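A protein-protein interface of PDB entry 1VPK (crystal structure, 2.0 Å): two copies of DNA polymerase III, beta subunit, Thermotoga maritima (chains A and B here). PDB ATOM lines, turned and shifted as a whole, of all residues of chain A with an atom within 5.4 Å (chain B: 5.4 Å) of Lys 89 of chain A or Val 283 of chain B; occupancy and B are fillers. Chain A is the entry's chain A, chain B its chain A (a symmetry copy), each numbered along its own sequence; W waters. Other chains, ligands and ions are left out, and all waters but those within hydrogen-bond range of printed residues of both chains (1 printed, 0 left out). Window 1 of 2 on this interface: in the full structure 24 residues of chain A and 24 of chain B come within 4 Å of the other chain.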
ATOM      1  N   GLY A  84     -24.143  26.857 -19.913  1.00  0.00           N
ATOM      2  CA  GLY A  84     -22.775  26.425 -20.112  1.00  0.00           C
ATOM      3  C   GLY A  84     -21.868  26.612 -18.919  1.00  0.00           C
ATOM      4  O   GLY A  84     -21.062  25.706 -18.580  1.00  0.00           O
ATOM      5  N   VAL A  86     -22.556  26.953 -15.517  1.00  0.00           N
ATOM      6  CA  VAL A  86     -22.897  26.069 -14.409  1.00  0.00           C
ATOM      7  C   VAL A  86     -22.500  24.591 -14.644  1.00  0.00           C
ATOM      8  O   VAL A  86     -21.977  23.953 -13.741  1.00  0.00           O
ATOM      9  CB  VAL A  86     -24.391  26.151 -14.104  1.00  0.00           C
ATOM     10  CG1 VAL A  86     -24.785  25.157 -13.053  1.00  0.00           C
ATOM     11  CG2 VAL A  86     -24.705  27.494 -13.589  1.00  0.00           C
ATOM     12  N   ILE A  87     -22.761  24.067 -15.844  1.00  0.00           N
ATOM     13  CA  ILE A  87     -22.465  22.672 -16.199  1.00  0.00           C
ATOM     14  C   ILE A  87     -20.965  22.425 -16.233  1.00  0.00           C
ATOM     15  O   ILE A  87     -20.483  21.398 -15.753  1.00  0.00           O
ATOM     16  CB  ILE A  87     -23.127  22.302 -17.565  1.00  0.00           C
ATOM     17  CG1 ILE A  87     -24.649  22.236 -17.421  1.00  0.00           C
ATOM     18  CG2 ILE A  87     -22.593  20.998 -18.095  1.00  0.00           C
ATOM     19  CD1 ILE A  87     -25.217  21.038 -16.622  1.00  0.00           C
ATOM     20  N   GLN A  88     -20.207  23.390 -16.764  1.00  0.00           N
ATOM     21  CA  GLN A  88     -18.771  23.321 -16.734  1.00  0.00           C
ATOM     22  C   GLN A  88     -18.235  23.272 -15.304  1.00  0.00           C
ATOM     23  O   GLN A  88     -17.411  22.422 -14.994  1.00  0.00           O
ATOM     24  CB  GLN A  88     -18.168  24.546 -17.419  1.00  0.00           C
ATOM     25  CG  GLN A  88     -18.067  24.417 -18.899  1.00  0.00           C
ATOM     26  CD  GLN A  88     -17.429  25.643 -19.478  1.00  0.00           C
ATOM     27  OE1 GLN A  88     -16.211  25.730 -19.539  1.00  0.00           O
ATOM     28  NE2 GLN A  88     -18.241  26.629 -19.854  1.00  0.00           N
ATOM     29  N   LYS A  89     -18.665  24.201 -14.458  1.00  0.00           N
ATOM     30  CA  LYS A  89     -18.256  24.213 -13.035  1.00  0.00           C
ATOM     31  C   LYS A  89     -18.657  22.927 -12.306  1.00  0.00           C
ATOM     32  O   LYS A  89     -17.888  22.373 -11.518  1.00  0.00           O
ATOM     33  CB  LYS A  89     -18.807  25.438 -12.313  1.00  0.00           C
ATOM     34  CG  LYS A  89     -18.205  26.737 -12.860  1.00  0.00           C
ATOM     35  CD  LYS A  89     -18.573  27.949 -12.028  1.00  0.00           C
ATOM     36  CE  LYS A  89     -17.990  29.239 -12.608  1.00  0.00           C
ATOM     37  NZ  LYS A  89     -17.913  30.309 -11.553  1.00  0.00           N
ATOM     38  N   MET A  90     -19.857  22.449 -12.617  1.00  0.00           N
ATOM     39  CA  MET A  90     -20.414  21.317 -11.959  1.00  0.00           C
ATOM     40  C   MET A  90     -19.617  20.051 -12.218  1.00  0.00           C
ATOM     41  O   MET A  90     -19.312  19.278 -11.256  1.00  0.00           O
ATOM     42  CB  MET A  90     -21.810  21.077 -12.477  1.00  0.00           C
ATOM     43  CG  MET A  90     -22.345  19.825 -11.986  1.00  0.00           C
ATOM     44  SD  MET A  90     -23.692  19.205 -12.896  1.00  0.00           S
ATOM     45  CE  MET A  90     -22.824  18.568 -14.306  1.00  0.00           C
ATOM     46  N   VAL A  91     -19.301  19.801 -13.498  1.00  0.00           N
ATOM     47  CA  VAL A  91     -18.669  18.528 -13.852  1.00  0.00           C
ATOM     48  C   VAL A  91     -17.297  18.388 -13.267  1.00  0.00           C
ATOM     49  O   VAL A  91     -16.866  17.248 -13.008  1.00  0.00           O
ATOM     50  CB  VAL A  91     -18.588  18.193 -15.386  1.00  0.00           C
ATOM     51  CG1 VAL A  91     -19.950  18.238 -15.956  1.00  0.00           C
ATOM     52  CG2 VAL A  91     -17.622  19.120 -16.116  1.00  0.00           C
ATOM     53  N   LYS A  92     -16.612  19.521 -13.089  1.00  0.00           N
ATOM     54  CA  LYS A  92     -15.263  19.532 -12.504  1.00  0.00           C
ATOM     55  C   LYS A  92     -15.234  19.182 -11.021  1.00  0.00           C
ATOM     56  O   LYS A  92     -14.178  18.887 -10.484  1.00  0.00           O
ATOM     57  CB  LYS A  92     -14.525  20.861 -12.793  1.00  0.00           C
ATOM     58  CG  LYS A  92     -14.294  21.047 -14.332  1.00  0.00           C
ATOM     59  CD  LYS A  92     -13.599  22.369 -14.719  1.00  0.00           C
ATOM     60  CE  LYS A  92     -14.116  22.852 -16.097  1.00  0.00           C
ATOM     61  NZ  LYS A  92     -13.190  23.799 -16.857  1.00  0.00           N
ATOM     62  N   VAL A  93     -16.388  19.179 -10.359  1.00  0.00           N
ATOM     63  CA  VAL A  93     -16.444  18.820  -8.935  1.00  0.00           C
ATOM     64  C   VAL A  93     -17.281  17.572  -8.581  1.00  0.00           C
ATOM     65  O   VAL A  93     -17.397  17.239  -7.402  1.00  0.00           O
ATOM     66  CB  VAL A  93     -16.932  20.042  -8.065  1.00  0.00           C
ATOM     67  CG1 VAL A  93     -15.984  21.252  -8.238  1.00  0.00           C
ATOM     68  CG2 VAL A  93     -18.351  20.440  -8.428  1.00  0.00           C
ATOM     69  N   PHE A 117     -27.091  17.463  -8.329  1.00  0.00           N
ATOM     70  CA  PHE A 117     -27.373  18.734  -8.957  1.00  0.00           C
ATOM     71  C   PHE A 117     -28.695  18.577  -9.736  1.00  0.00           C
ATOM     72  O   PHE A 117     -28.924  17.545 -10.355  1.00  0.00           O
ATOM     73  CB  PHE A 117     -26.262  19.128  -9.912  1.00  0.00           C
ATOM     74  CG  PHE A 117     -24.998  19.662  -9.249  1.00  0.00           C
ATOM     75  CD1 PHE A 117     -24.845  21.009  -8.974  1.00  0.00           C
ATOM     76  CD2 PHE A 117     -23.918  18.798  -8.977  1.00  0.00           C
ATOM     77  CE1 PHE A 117     -23.681  21.511  -8.404  1.00  0.00           C
ATOM     78  CE2 PHE A 117     -22.736  19.298  -8.411  1.00  0.00           C
ATOM     79  CZ  PHE A 117     -22.612  20.648  -8.142  1.00  0.00           C
ATOM     80  N   LEU B 278     -18.274  22.042   0.335  1.00  0.00           N
ATOM     81  CA  LEU B 278     -18.527  23.491   0.148  1.00  0.00           C
ATOM     82  C   LEU B 278     -18.253  23.936  -1.285  1.00  0.00           C
ATOM     83  O   LEU B 278     -19.065  24.639  -1.906  1.00  0.00           O
ATOM     84  CB  LEU B 278     -17.719  24.318   1.164  1.00  0.00           C
ATOM     85  CG  LEU B 278     -18.352  24.189   2.552  1.00  0.00           C
ATOM     86  CD1 LEU B 278     -17.404  24.603   3.651  1.00  0.00           C
ATOM     87  CD2 LEU B 278     -19.672  24.965   2.678  1.00  0.00           C
ATOM     88  N   LYS B 279     -17.147  23.477  -1.857  1.00  0.00           N
ATOM     89  CA  LYS B 279     -16.869  23.780  -3.261  1.00  0.00           C
ATOM     90  C   LYS B 279     -17.991  23.323  -4.234  1.00  0.00           C
ATOM     91  O   LYS B 279     -18.361  24.048  -5.170  1.00  0.00           O
ATOM     92  CB  LYS B 279     -15.554  23.163  -3.700  1.00  0.00           C
ATOM     93  CG  LYS B 279     -14.297  23.879  -3.230  1.00  0.00           C
ATOM     94  CD  LYS B 279     -13.138  23.492  -4.203  1.00  0.00           C
ATOM     95  N   ARG B 280     -18.531  22.130  -4.003  1.00  0.00           N
ATOM     96  CA  ARG B 280     -19.626  21.605  -4.835  1.00  0.00           C
ATOM     97  C   ARG B 280     -20.875  22.495  -4.735  1.00  0.00           C
ATOM     98  O   ARG B 280     -21.457  22.849  -5.756  1.00  0.00           O
ATOM     99  CB  ARG B 280     -19.930  20.109  -4.513  1.00  0.00           C
ATOM    100  CG  ARG B 280     -18.736  19.243  -4.851  1.00  0.00           C
ATOM    101  CD  ARG B 280     -18.906  17.744  -4.735  1.00  0.00           C
ATOM    102  NE  ARG B 280     -19.079  17.258  -3.374  1.00  0.00           N
ATOM    103  CZ  ARG B 280     -18.135  16.642  -2.634  1.00  0.00           C
ATOM    104  NH1 ARG B 280     -16.914  16.425  -3.084  1.00  0.00           N
ATOM    105  NH2 ARG B 280     -18.425  16.222  -1.435  1.00  0.00           N
ATOM    106  N   VAL B 281     -21.277  22.890  -3.528  1.00  0.00           N
ATOM    107  CA  VAL B 281     -22.502  23.636  -3.388  1.00  0.00           C
ATOM    108  C   VAL B 281     -22.336  25.080  -3.837  1.00  0.00           C
ATOM    109  O   VAL B 281     -23.299  25.697  -4.227  1.00  0.00           O
ATOM    110  CB  VAL B 281     -23.153  23.546  -1.958  1.00  0.00           C
ATOM    111  CG1 VAL B 281     -23.446  22.058  -1.576  1.00  0.00           C
ATOM    112  CG2 VAL B 281     -22.284  24.214  -0.896  1.00  0.00           C
ATOM    113  N   MET B 282     -21.106  25.584  -3.820  1.00  0.00           N
ATOM    114  CA  MET B 282     -20.804  26.920  -4.311  1.00  0.00           C
ATOM    115  C   MET B 282     -20.980  27.061  -5.787  1.00  0.00           C
ATOM    116  O   MET B 282     -21.202  28.162  -6.286  1.00  0.00           O
ATOM    117  CB  MET B 282     -19.416  27.383  -3.869  1.00  0.00           C
ATOM    118  CG  MET B 282     -19.486  27.771  -2.399  1.00  0.00           C
ATOM    119  SD  MET B 282     -18.014  28.327  -1.536  1.00  0.00           S
ATOM    120  CE  MET B 282     -16.874  26.963  -1.386  1.00  0.00           C
ATOM    121  N   VAL B 283     -20.947  25.959  -6.501  1.00  0.00           N
ATOM    122  CA  VAL B 283     -21.309  26.002  -7.903  1.00  0.00           C
ATOM    123  C   VAL B 283     -22.684  26.689  -8.058  1.00  0.00           C
ATOM    124  O   VAL B 283     -22.876  27.479  -8.975  1.00  0.00           O
ATOM    125  CB  VAL B 283     -21.304  24.608  -8.536  1.00  0.00           C
ATOM    126  CG1 VAL B 283     -21.941  24.658  -9.964  1.00  0.00           C
ATOM    127  CG2 VAL B 283     -19.902  24.082  -8.608  1.00  0.00           C
ATOM    128  N   ILE B 284     -23.622  26.389  -7.156  1.00  0.00           N
ATOM    129  CA  ILE B 284     -24.956  26.994  -7.189  1.00  0.00           C
ATOM    130  C   ILE B 284     -25.037  28.251  -6.315  1.00  0.00           C
ATOM    131  O   ILE B 284     -25.640  29.224  -6.720  1.00  0.00           O
ATOM    132  CB  ILE B 284     -26.082  25.981  -6.821  1.00  0.00           C
ATOM    133  CG1 ILE B 284     -26.207  24.933  -7.928  1.00  0.00           C
ATOM    134  CG2 ILE B 284     -27.456  26.708  -6.567  1.00  0.00           C
ATOM    135  CD1 ILE B 284     -26.510  25.434  -9.279  1.00  0.00           C
ATOM    136  N   ALA B 285     -24.397  28.227  -5.143  1.00  0.00           N
ATOM    137  CA  ALA B 285     -24.471  29.361  -4.227  1.00  0.00           C
ATOM    138  C   ALA B 285     -23.889  30.667  -4.810  1.00  0.00           C
ATOM    139  O   ALA B 285     -24.433  31.773  -4.558  1.00  0.00           O
ATOM    140  CB  ALA B 285     -23.823  29.013  -2.889  1.00  0.00           C
ATOM    141  N   SER B 286     -22.829  30.543  -5.604  1.00  0.00           N
ATOM    142  CA  SER B 286     -22.154  31.704  -6.200  1.00  0.00           C
ATOM    143  C   SER B 286     -22.985  32.394  -7.241  1.00  0.00           C
ATOM    144  O   SER B 286     -22.707  33.552  -7.595  1.00  0.00           O
ATOM    145  CB  SER B 286     -20.791  31.324  -6.782  1.00  0.00           C
ATOM    146  OG  SER B 286     -19.861  31.140  -5.692  1.00  0.00           O
ATOM    147  N   LYS B 287     -24.014  31.701  -7.727  1.00  0.00           N
ATOM    148  CA  LYS B 287     -24.920  32.282  -8.686  1.00  0.00           C
ATOM    149  C   LYS B 287     -25.810  33.386  -8.107  1.00  0.00           C
ATOM    150  O   LYS B 287     -26.234  34.263  -8.844  1.00  0.00           O
ATOM    151  CB  LYS B 287     -25.768  31.192  -9.361  1.00  0.00           C
ATOM    152  CG  LYS B 287     -25.011  30.392 -10.402  1.00  0.00           C
ATOM    153  CD  LYS B 287     -24.915  31.202 -11.701  1.00  0.00           C
ATOM    154  CE  LYS B 287     -23.698  30.838 -12.535  1.00  0.00           C
ATOM    155  NZ  LYS B 287     -23.285  31.985 -13.367  1.00  0.00           N
HETATM  156  O   HOH W   1     -15.431  17.333  -5.521  1.00  0.00           O
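Of the 10 printed residues of chain A, 4 touch a printed residue of chain B.
Hydrophobic or aromatic side chains of chain A that line the printed part of chain B: Val 86, Val 93 and Phe 117.
Hydrophobic or aromatic side chains of chain B that line the printed part of chain A: Val 283.
Among the printed residues, no Asp or Glu carboxylate lies within 4 Å of a Lys or Arg side-chain nitrogen of the other chain.
No position is printed for both chains.
Of the 7 pairs that touch across the chains among the printed residues, none has its exchanged pair printed and touching as well.
Of the printed residues of chain B, Lys 89 of chain A touches Val 283.
Of chain A, only Val 86 (3.8 Å), Lys 89 (3.9 Å), Val 93 (3.96 Å) and Phe 117 (3.9 Å) come within 4 Å of Val 283 of chain B.
Printed residues of chain B within 4 Å of Val 86 of chain A: Val 283 (3.8 Å) and Lys 287 (3.6 Å).
Printed residues of chain A within 4 Å of Lys 287 of chain B: Val 86.
Printed residues of chain A within 4 Å of Arg 280 of chain B: Val 93 and Phe 117.
Of the printed residues of chain B, Phe 117 of chain A touches Arg 280 (3.4 Å) and Val 283 (3.9 Å).
Of the printed residues of chain B, Val 93 of chain A touches Arg 280 (3.1 Å) and Val 283 (3.96 Å).
The nearest printed residue of chain B that does not touch Lys 89 of chain A is Ser 286 of chain B (5.7 Å).
Val 86 of chain A touches Val 283 of chain B.
CE of Lys 287 of chain B touches CG2 of Val 86 of chain A, at 3.6 Å.
Val 283 of chain B touches Lys 89 of chain A (CG2 to O, 3.9 Å).
Val 93 of chain A touches Arg 280 of chain B (O to CD, 3.1 Å).
CG2 of Val 283 of chain B touches CG2 of Val 93 of chain A, at 3.96 Å.
CZ of Phe 117 of chain A touches O of Arg 280 of chain B (3.4 Å).
Phe 117 of chain A touches Val 283 of chain B (CE1 to CB, 3.9 Å).
Water W1 lies within hydrogen-bond range of the backbone carbonyl oxygen of Val 93 of chain A (2.7 Å) and the guanidinium group of Arg 280 of chain B (3.0 Å).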
